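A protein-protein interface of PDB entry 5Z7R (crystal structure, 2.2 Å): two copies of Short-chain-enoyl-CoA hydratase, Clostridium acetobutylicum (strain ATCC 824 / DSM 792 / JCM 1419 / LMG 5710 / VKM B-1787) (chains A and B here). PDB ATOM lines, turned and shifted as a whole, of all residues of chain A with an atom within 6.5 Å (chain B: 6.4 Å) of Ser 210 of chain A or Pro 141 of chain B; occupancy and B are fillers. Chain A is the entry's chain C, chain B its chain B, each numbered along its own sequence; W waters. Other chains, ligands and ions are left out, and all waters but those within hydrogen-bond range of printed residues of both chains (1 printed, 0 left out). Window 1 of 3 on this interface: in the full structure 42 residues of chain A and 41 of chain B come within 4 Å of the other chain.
N of Gly 145 of chain B sits at hydrogen-bond distance from OE1 of Glu 229 of chain A (2.9 Å).
The backbone NH (N) of Gly 144 of chain B is in hydrogen-bond range of the side-chain carboxylate (OE2) of Glu 229 of chain A, at 2.6 Å.
OE1 of Glu 229 of chain A lies within hydrogen-bond range of OG1 of Thr 146 of chain B, at 2.6 Å.
OE2 of Glu 229 of chain A lies close to O of Gly 142 of chain B, at 3.2 Å.
The backbone NH of Phe 143 of chain B lies within hydrogen-bond range of the side-chain carboxylate of Glu 229 of chain A.
The backbone NH (N) of Gly 142 of chain B is in hydrogen-bond range of the side-chain carboxylate (OE2) of Glu 114 of chain B, 3.1 Å away.
The backbone NH (N) of Ile 139 of chain B is in hydrogen-bond range of the backbone carbonyl oxygen (O) of Glu 134 of chain B (3.1 Å).
OE2 of Glu 114 of chain B is in hydrogen-bond range of N of Phe 143 of chain B (2.7 Å).
The backbone NH (N) of Gly 144 of chain B lies within hydrogen-bond range of the side-chain carboxylate (OE2) of Glu 114 of chain B (3.4 Å).
The side-chain carboxylate (OE2) of Glu 114 of chain B is in hydrogen-bond range of the backbone NH (N) of Gly 145 of chain B.
The side-chain hydroxyl (OG) of Ser 210 of chain A sits at hydrogen-bond distance from the backbone carbonyl oxygen (O) of Ala 206 of chain A, 2.6 Å away.
Among the printed residues, pairs that only touch across the chains: Val 207 of chain A with Val 135 of chain B (3.3 Å), Ala 206 of chain A with Val 135 of chain B (3.4 Å), Phe 233 of chain A with Thr 140 of chain B (3.4 Å), Glu 229 of chain A with Pro 141 of chain B (3.5 Å), Ser 210 of chain A with Thr 140 of chain B (3.5 Å), Ala 206 of chain A with Ile 139 of chain B (3.5 Å), Ile 214 of chain A with Thr 146 of chain B (3.5 Å), Phe 233 of chain A with Gly 142 of chain B (3.6 Å), Lys 211 of chain A with Phe 163 of chain B (3.7 Å), Ala 213 of chain A with Thr 146 of chain B (3.8 Å), Ser 210 of chain A with Pro 141 of chain B (3.8 Å), Ser 210 of chain A with Ile 162 of chain B (3.8 Å), Phe 233 of chain A with Ile 139 of chain B (3.8 Å), Phe 233 of chain A with Pro 141 of chain B (3.9 Å), Ala 206 of chain A with Thr 140 of chain B (3.9 Å), Ile 214 of chain A with Ile 162 of chain B (3.9 Å) and Leu 209 of chain A with Thr 140 of chain B (3.9 Å).
Of chain A, only Ser 210, Glu 229 and Phe 233 come within 4 Å of Pro 141 of chain B.
Printed residues of chain A within 4 Å of Gly 144 of chain B: Glu 229 (2.6 Å).
Of the printed residues of chain A, Ile 139 of chain B touches Ala 206 and Phe 233.
Printed residues of chain A within 4 Å of Thr 140 of chain B: Ala 206, Leu 209, Ser 210 and Phe 233.
Of the printed residues of chain A, Ile 162 of chain B touches Ser 210 (3.8 Å) and Ile 214 (3.9 Å).
Ser 230 of chain A touches none of the printed residues of chain B.
Asn 215 of chain A touches none of the printed residues of chain B.
The nearest residue of chain B that does not touch Ser 210 of chain A is Val 135 of chain B (4.2 Å).
The nearest residue of chain A that does not touch Pro 141 of chain B is Ala 206 of chain A (6.0 Å).
The nearest printed residue of chain B that does not touch Lys 211 of chain A is Ile 162 of chain B (6.0 Å).
Of the 15 printed residues of chain A, 9 touch a printed residue of chain B.
Hydrophobic or aromatic side chains of chain A within 4 Å of the printed part of chain B: Ala 206, Val 207, Leu 209, Ala 213, Ile 214 and Phe 233.
Among the printed residues, 22 pairs touch across the chains.
Among the printed residues, no Asp or Glu carboxylate lies within 4 Å of a Lys or Arg side-chain nitrogen of the other chain.
No position is printed for both chains.
Of the 22 pairs that touch across the chains among the printed residues, none has its exchanged pair printed and touching as well.
Water W1 lies within hydrogen-bond range of O of Gly 142 of chain B (2.6 Å), OE2 of Glu 229 of chain A (2.7 Å) and OG of Ser 230 of chain A (2.7 Å).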
ATOM      1  N   VAL A 205      25.643 -32.422  18.695  1.00  0.00           N
ATOM      2  CA  VAL A 205      24.260 -31.946  18.774  1.00  0.00           C
ATOM      3  C   VAL A 205      24.017 -31.067  17.573  1.00  0.00           C
ATOM      4  O   VAL A 205      22.965 -31.126  16.968  1.00  0.00           O
ATOM      5  CB  VAL A 205      23.976 -31.168  20.111  1.00  0.00           C
ATOM      6  CG1 VAL A 205      22.635 -30.444  20.094  1.00  0.00           C
ATOM      7  CG2 VAL A 205      23.965 -32.126  21.290  1.00  0.00           C
ATOM      8  N   ALA A 206      25.016 -30.282  17.196  1.00  0.00           N
ATOM      9  CA  ALA A 206      24.885 -29.396  16.060  1.00  0.00           C
ATOM     10  C   ALA A 206      24.725 -30.167  14.720  1.00  0.00           C
ATOM     11  O   ALA A 206      23.931 -29.800  13.869  1.00  0.00           O
ATOM     12  CB  ALA A 206      26.082 -28.464  15.993  1.00  0.00           C
ATOM     13  N   VAL A 207      25.507 -31.212  14.557  1.00  0.00           N
ATOM     14  CA  VAL A 207      25.419 -32.062  13.423  1.00  0.00           C
ATOM     15  C   VAL A 207      24.067 -32.745  13.374  1.00  0.00           C
ATOM     16  O   VAL A 207      23.440 -32.820  12.319  1.00  0.00           O
ATOM     17  CB  VAL A 207      26.520 -33.140  13.445  1.00  0.00           C
ATOM     18  CG1 VAL A 207      26.316 -34.146  12.335  1.00  0.00           C
ATOM     19  CG2 VAL A 207      27.900 -32.512  13.291  1.00  0.00           C
ATOM     20  N   LYS A 208      23.656 -33.283  14.512  1.00  0.00           N
ATOM     21  CA  LYS A 208      22.395 -33.980  14.661  1.00  0.00           C
ATOM     22  C   LYS A 208      21.235 -33.040  14.322  1.00  0.00           C
ATOM     23  O   LYS A 208      20.332 -33.400  13.596  1.00  0.00           O
ATOM     24  CB  LYS A 208      22.297 -34.458  16.100  1.00  0.00           C
ATOM     25  CG  LYS A 208      20.935 -34.895  16.592  1.00  0.00           C
ATOM     26  CD  LYS A 208      21.012 -35.497  18.006  1.00  0.00           C
ATOM     27  CE  LYS A 208      21.959 -36.708  18.035  1.00  0.00           C
ATOM     28  NZ  LYS A 208      21.501 -37.970  18.714  1.00  0.00           N
ATOM     29  N   LEU A 209      21.269 -31.825  14.824  1.00  0.00           N
ATOM     30  CA  LEU A 209      20.167 -30.911  14.585  1.00  0.00           C
ATOM     31  C   LEU A 209      20.195 -30.294  13.158  1.00  0.00           C
ATOM     32  O   LEU A 209      19.126 -29.970  12.571  1.00  0.00           O
ATOM     33  CB  LEU A 209      20.127 -29.841  15.668  1.00  0.00           C
ATOM     34  CG  LEU A 209      19.796 -30.389  17.060  1.00  0.00           C
ATOM     35  CD1 LEU A 209      19.857 -29.266  18.086  1.00  0.00           C
ATOM     36  CD2 LEU A 209      18.436 -31.025  17.170  1.00  0.00           C
ATOM     37  N   SER A 210      21.390 -30.163  12.597  1.00  0.00           N
ATOM     38  CA  SER A 210      21.508 -29.752  11.225  1.00  0.00           C
ATOM     39  C   SER A 210      20.900 -30.824  10.339  1.00  0.00           C
ATOM     40  O   SER A 210      20.121 -30.537   9.418  1.00  0.00           O
ATOM     41  CB  SER A 210      22.966 -29.536  10.869  1.00  0.00           C
ATOM     42  OG  SER A 210      23.526 -28.487  11.654  1.00  0.00           O
ATOM     43  N   LYS A 211      21.207 -32.088  10.613  1.00  0.00           N
ATOM     44  CA  LYS A 211      20.566 -33.127   9.820  1.00  0.00           C
ATOM     45  C   LYS A 211      19.025 -33.087   9.919  1.00  0.00           C
ATOM     46  O   LYS A 211      18.351 -33.231   8.944  1.00  0.00           O
ATOM     47  CB  LYS A 211      21.086 -34.529  10.144  1.00  0.00           C
ATOM     48  CG  LYS A 211      20.539 -35.581   9.187  1.00  0.00           C
ATOM     49  CD  LYS A 211      21.020 -37.003   9.453  1.00  0.00           C
ATOM     50  CE  LYS A 211      20.179 -38.025   8.685  1.00  0.00           C
ATOM     51  NZ  LYS A 211      20.912 -39.295   8.520  1.00  0.00           N
ATOM     52  N   GLN A 212      18.466 -32.987  11.103  1.00  0.00           N
ATOM     53  CA  GLN A 212      17.037 -32.922  11.210  1.00  0.00           C
ATOM     54  C   GLN A 212      16.531 -31.747  10.390  1.00  0.00           C
ATOM     55  O   GLN A 212      15.643 -31.907   9.575  1.00  0.00           O
ATOM     56  CB  GLN A 212      16.598 -32.723  12.650  1.00  0.00           C
ATOM     57  CG  GLN A 212      15.089 -32.648  12.800  1.00  0.00           C
ATOM     58  CD  GLN A 212      14.407 -34.001  12.805  1.00  0.00           C
ATOM     59  OE1 GLN A 212      14.657 -34.858  11.956  1.00  0.00           O
ATOM     60  NE2 GLN A 212      13.537 -34.204  13.772  1.00  0.00           N
ATOM     61  N   ALA A 213      17.097 -30.568  10.592  1.00  0.00           N
ATOM     62  CA  ALA A 213      16.594 -29.389   9.926  1.00  0.00           C
ATOM     63  C   ALA A 213      16.531 -29.564   8.415  1.00  0.00           C
ATOM     64  O   ALA A 213      15.569 -29.104   7.723  1.00  0.00           O
ATOM     65  CB  ALA A 213      17.475 -28.181  10.244  1.00  0.00           C
ATOM     66  N   ILE A 214      17.605 -30.147   7.898  1.00  0.00           N
ATOM     67  CA  ILE A 214      17.742 -30.386   6.472  1.00  0.00           C
ATOM     68  C   ILE A 214      16.699 -31.404   6.045  1.00  0.00           C
ATOM     69  O   ILE A 214      15.924 -31.133   5.179  1.00  0.00           O
ATOM     70  CB  ILE A 214      19.144 -30.866   6.090  1.00  0.00           C
ATOM     71  CG1 ILE A 214      20.157 -29.753   6.344  1.00  0.00           C
ATOM     72  CG2 ILE A 214      19.185 -31.279   4.589  1.00  0.00           C
ATOM     73  CD1 ILE A 214      21.582 -30.235   6.348  1.00  0.00           C
ATOM     74  N   ASN A 215      16.655 -32.557   6.684  1.00  0.00           N
ATOM     75  CA  ASN A 215      15.658 -33.523   6.309  1.00  0.00           C
ATOM     76  C   ASN A 215      14.244 -32.974   6.322  1.00  0.00           C
ATOM     77  O   ASN A 215      13.499 -33.179   5.358  1.00  0.00           O
ATOM     78  CB  ASN A 215      15.721 -34.758   7.198  1.00  0.00           C
ATOM     79  CG  ASN A 215      16.826 -35.714   6.782  1.00  0.00           C
ATOM     80  OD1 ASN A 215      17.347 -35.642   5.677  1.00  0.00           O
ATOM     81  ND2 ASN A 215      17.166 -36.617   7.665  1.00  0.00           N
ATOM     82  N   GLU A 229      14.437 -24.208  11.430  1.00  0.00           N
ATOM     83  CA  GLU A 229      15.830 -23.971  11.656  1.00  0.00           C
ATOM     84  C   GLU A 229      16.064 -23.231  12.954  1.00  0.00           C
ATOM     85  O   GLU A 229      16.947 -23.614  13.748  1.00  0.00           O
ATOM     86  CB  GLU A 229      16.439 -23.158  10.510  1.00  0.00           C
ATOM     87  CG  GLU A 229      17.964 -23.038  10.574  1.00  0.00           C
ATOM     88  CD  GLU A 229      18.557 -22.080   9.567  1.00  0.00           C
ATOM     89  OE1 GLU A 229      19.054 -22.578   8.514  1.00  0.00           O
ATOM     90  OE2 GLU A 229      18.563 -20.841   9.818  1.00  0.00           O
ATOM     91  N   SER A 230      15.320 -22.143  13.149  1.00  0.00           N
ATOM     92  CA  SER A 230      15.563 -21.295  14.316  1.00  0.00           C
ATOM     93  C   SER A 230      15.245 -22.009  15.622  1.00  0.00           C
ATOM     94  O   SER A 230      15.887 -21.739  16.616  1.00  0.00           O
ATOM     95  CB  SER A 230      14.841 -19.968  14.209  1.00  0.00           C
ATOM     96  OG  SER A 230      15.563 -19.139  13.337  1.00  0.00           O
ATOM     97  N   ALA A 232      15.779 -25.238  16.144  1.00  0.00           N
ATOM     98  CA  ALA A 232      16.952 -26.073  16.244  1.00  0.00           C
ATOM     99  C   ALA A 232      18.218 -25.293  16.566  1.00  0.00           C
ATOM    100  O   ALA A 232      18.999 -25.743  17.382  1.00  0.00           O
ATOM    101  CB  ALA A 232      17.163 -26.879  14.960  1.00  0.00           C
ATOM    102  N   PHE A 233      18.423 -24.171  15.919  1.00  0.00           N
ATOM    103  CA  PHE A 233      19.502 -23.275  16.241  1.00  0.00           C
ATOM    104  C   PHE A 233      19.494 -22.935  17.758  1.00  0.00           C
ATOM    105  O   PHE A 233      20.472 -23.144  18.476  1.00  0.00           O
ATOM    106  CB  PHE A 233      19.299 -22.024  15.405  1.00  0.00           C
ATOM    107  CG  PHE A 233      20.423 -21.038  15.455  1.00  0.00           C
ATOM    108  CD1 PHE A 233      21.715 -21.405  15.117  1.00  0.00           C
ATOM    109  CD2 PHE A 233      20.169 -19.703  15.730  1.00  0.00           C
ATOM    110  CE1 PHE A 233      22.727 -20.465  15.096  1.00  0.00           C
ATOM    111  CE2 PHE A 233      21.180 -18.757  15.748  1.00  0.00           C
ATOM    112  CZ  PHE A 233      22.462 -19.134  15.417  1.00  0.00           C
ATOM    113  N   GLU B 114      25.186 -17.871   3.647  1.00  0.00           N
ATOM    114  CA  GLU B 114      23.759 -17.744   3.849  1.00  0.00           C
ATOM    115  C   GLU B 114      23.115 -16.479   3.194  1.00  0.00           C
ATOM    116  O   GLU B 114      22.004 -16.573   2.672  1.00  0.00           O
ATOM    117  CB  GLU B 114      23.477 -17.808   5.325  1.00  0.00           C
ATOM    118  CG  GLU B 114      23.417 -19.220   5.868  1.00  0.00           C
ATOM    119  CD  GLU B 114      23.439 -19.249   7.386  1.00  0.00           C
ATOM    120  OE1 GLU B 114      24.267 -18.495   7.946  1.00  0.00           O
ATOM    121  OE2 GLU B 114      22.651 -19.994   8.032  1.00  0.00           O
ATOM    122  N   GLN B 132      30.059 -23.437   5.361  1.00  0.00           N
ATOM    123  CA  GLN B 132      29.310 -23.319   6.576  1.00  0.00           C
ATOM    124  C   GLN B 132      30.097 -23.932   7.763  1.00  0.00           C
ATOM    125  O   GLN B 132      29.946 -25.110   8.047  1.00  0.00           O
ATOM    126  CB  GLN B 132      28.005 -24.116   6.428  1.00  0.00           C
ATOM    127  CG  GLN B 132      27.068 -23.665   5.313  1.00  0.00           C
ATOM    128  CD  GLN B 132      26.357 -22.344   5.583  1.00  0.00           C
ATOM    129  OE1 GLN B 132      26.168 -21.906   6.745  1.00  0.00           O
ATOM    130  NE2 GLN B 132      25.950 -21.705   4.513  1.00  0.00           N
ATOM    131  N   GLU B 134      29.589 -23.535  10.953  1.00  0.00           N
ATOM    132  CA  GLU B 134      28.802 -23.455  12.183  1.00  0.00           C
ATOM    133  C   GLU B 134      28.839 -24.699  13.070  1.00  0.00           C
ATOM    134  O   GLU B 134      28.748 -24.605  14.284  1.00  0.00           O
ATOM    135  CB  GLU B 134      27.322 -23.107  11.891  1.00  0.00           C
ATOM    136  CG  GLU B 134      27.089 -21.662  11.441  1.00  0.00           C
ATOM    137  CD  GLU B 134      27.202 -21.515   9.966  1.00  0.00           C
ATOM    138  OE1 GLU B 134      26.790 -20.469   9.403  1.00  0.00           O
ATOM    139  OE2 GLU B 134      27.690 -22.499   9.343  1.00  0.00           O
ATOM    140  N   VAL B 135      28.951 -25.866  12.493  1.00  0.00           N
ATOM    141  CA  VAL B 135      28.780 -27.069  13.275  1.00  0.00           C
ATOM    142  C   VAL B 135      30.076 -27.344  14.113  1.00  0.00           C
ATOM    143  O   VAL B 135      30.075 -28.069  15.138  1.00  0.00           O
ATOM    144  CB  VAL B 135      28.385 -28.191  12.315  1.00  0.00           C
ATOM    145  CG1 VAL B 135      29.603 -28.919  11.798  1.00  0.00           C
ATOM    146  CG2 VAL B 135      27.455 -29.141  12.976  1.00  0.00           C
ATOM    147  N   ILE B 139      26.904 -25.090  16.736  1.00  0.00           N
ATOM    148  CA  ILE B 139      25.562 -24.695  16.256  1.00  0.00           C
ATOM    149  C   ILE B 139      25.233 -25.159  14.830  1.00  0.00           C
ATOM    150  O   ILE B 139      26.108 -25.522  14.043  1.00  0.00           O
ATOM    151  CB  ILE B 139      25.391 -23.166  16.257  1.00  0.00           C
ATOM    152  CG1 ILE B 139      26.644 -22.513  15.677  1.00  0.00           C
ATOM    153  CG2 ILE B 139      25.077 -22.692  17.674  1.00  0.00           C
ATOM    154  CD1 ILE B 139      26.507 -21.065  15.243  1.00  0.00           C
ATOM    155  N   THR B 140      23.951 -25.089  14.497  1.00  0.00           N
ATOM    156  CA  THR B 140      23.502 -25.215  13.125  1.00  0.00           C
ATOM    157  C   THR B 140      23.796 -23.901  12.425  1.00  0.00           C
ATOM    158  O   THR B 140      24.043 -22.892  13.073  1.00  0.00           O
ATOM    159  CB  THR B 140      21.992 -25.493  13.047  1.00  0.00           C
ATOM    160  OG1 THR B 140      21.243 -24.354  13.469  1.00  0.00           O
ATOM    161  CG2 THR B 140      21.612 -26.633  13.952  1.00  0.00           C
ATOM    162  N   PRO B 141      23.805 -23.917  11.079  1.00  0.00           N
ATOM    163  CA  PRO B 141      23.564 -22.673  10.387  1.00  0.00           C
ATOM    164  C   PRO B 141      22.356 -22.013  11.003  1.00  0.00           C
ATOM    165  O   PRO B 141      21.420 -22.703  11.456  1.00  0.00           O
ATOM    166  CB  PRO B 141      23.232 -23.110   8.967  1.00  0.00           C
ATOM    167  CG  PRO B 141      23.909 -24.434   8.805  1.00  0.00           C
ATOM    168  CD  PRO B 141      24.024 -25.050  10.160  1.00  0.00           C
ATOM    169  N   GLY B 142      22.409 -20.690  11.083  1.00  0.00           N
ATOM    170  CA  GLY B 142      21.373 -19.959  11.766  1.00  0.00           C
ATOM    171  C   GLY B 142      20.621 -18.940  10.947  1.00  0.00           C
ATOM    172  O   GLY B 142      19.685 -18.354  11.447  1.00  0.00           O
ATOM    173  N   PHE B 143      21.062 -18.680   9.730  1.00  0.00           N
ATOM    174  CA  PHE B 143      20.403 -17.705   8.871  1.00  0.00           C
ATOM    175  C   PHE B 143      19.913 -18.353   7.584  1.00  0.00           C
ATOM    176  O   PHE B 143      20.073 -17.787   6.518  1.00  0.00           O
ATOM    177  CB  PHE B 143      21.355 -16.543   8.521  1.00  0.00           C
ATOM    178  CG  PHE B 143      21.848 -15.729   9.720  1.00  0.00           C
ATOM    179  CD1 PHE B 143      21.184 -15.731  10.949  1.00  0.00           C
ATOM    180  CD2 PHE B 143      22.957 -14.910   9.579  1.00  0.00           C
ATOM    181  CE1 PHE B 143      21.646 -14.978  12.020  1.00  0.00           C
ATOM    182  CE2 PHE B 143      23.419 -14.150  10.639  1.00  0.00           C
ATOM    183  CZ  PHE B 143      22.773 -14.185  11.864  1.00  0.00           C
ATOM    184  N   GLY B 144      19.326 -19.540   7.703  1.00  0.00           N
ATOM    185  CA  GLY B 144      18.737 -20.260   6.561  1.00  0.00           C
ATOM    186  C   GLY B 144      19.550 -21.374   5.931  1.00  0.00           C
ATOM    187  O   GLY B 144      19.047 -22.078   5.070  1.00  0.00           O
ATOM    188  N   GLY B 145      20.790 -21.571   6.382  1.00  0.00           N
ATOM    189  CA  GLY B 145      21.765 -22.337   5.639  1.00  0.00           C
ATOM    190  C   GLY B 145      21.285 -23.745   5.554  1.00  0.00           C
ATOM    191  O   GLY B 145      21.582 -24.459   4.596  1.00  0.00           O
ATOM    192  N   THR B 146      20.488 -24.152   6.530  1.00  0.00           N
ATOM    193  CA  THR B 146      20.019 -25.533   6.547  1.00  0.00           C
ATOM    194  C   THR B 146      18.920 -25.730   5.522  1.00  0.00           C
ATOM    195  O   THR B 146      18.402 -26.839   5.376  1.00  0.00           O
ATOM    196  CB  THR B 146      19.439 -25.949   7.929  1.00  0.00           C
ATOM    197  OG1 THR B 146      18.337 -25.078   8.281  1.00  0.00           O
ATOM    198  CG2 THR B 146      20.527 -25.929   9.061  1.00  0.00           C
ATOM    199  N   ILE B 162      27.679 -28.934   5.210  1.00  0.00           N
ATOM    200  CA  ILE B 162      27.206 -28.571   6.518  1.00  0.00           C
ATOM    201  C   ILE B 162      27.765 -29.516   7.618  1.00  0.00           C
ATOM    202  O   ILE B 162      28.156 -29.016   8.658  1.00  0.00           O
ATOM    203  CB  ILE B 162      25.672 -28.444   6.552  1.00  0.00           C
ATOM    204  CG1 ILE B 162      25.259 -27.187   5.790  1.00  0.00           C
ATOM    205  CG2 ILE B 162      25.136 -28.362   7.976  1.00  0.00           C
ATOM    206  CD1 ILE B 162      23.757 -27.062   5.562  1.00  0.00           C
ATOM    207  N   PHE B 163      27.783 -30.836   7.413  1.00  0.00           N
ATOM    208  CA  PHE B 163      28.291 -31.751   8.431  1.00  0.00           C
ATOM    209  C   PHE B 163      29.801 -31.689   8.591  1.00  0.00           C
ATOM    210  O   PHE B 163      30.290 -31.849   9.682  1.00  0.00           O
ATOM    211  CB  PHE B 163      27.922 -33.217   8.178  1.00  0.00           C
ATOM    212  CG  PHE B 163      26.455 -33.495   7.992  1.00  0.00           C
ATOM    213  CD1 PHE B 163      25.466 -32.678   8.533  1.00  0.00           C
ATOM    214  CD2 PHE B 163      26.068 -34.642   7.326  1.00  0.00           C
ATOM    215  CE1 PHE B 163      24.125 -32.980   8.359  1.00  0.00           C
ATOM    216  CE2 PHE B 163      24.743 -34.957   7.168  1.00  0.00           C
ATOM    217  CZ  PHE B 163      23.764 -34.125   7.684  1.00  0.00           C
HETATM  218  O   HOH W   1      17.948 -20.026  12.311  1.00  0.00           O
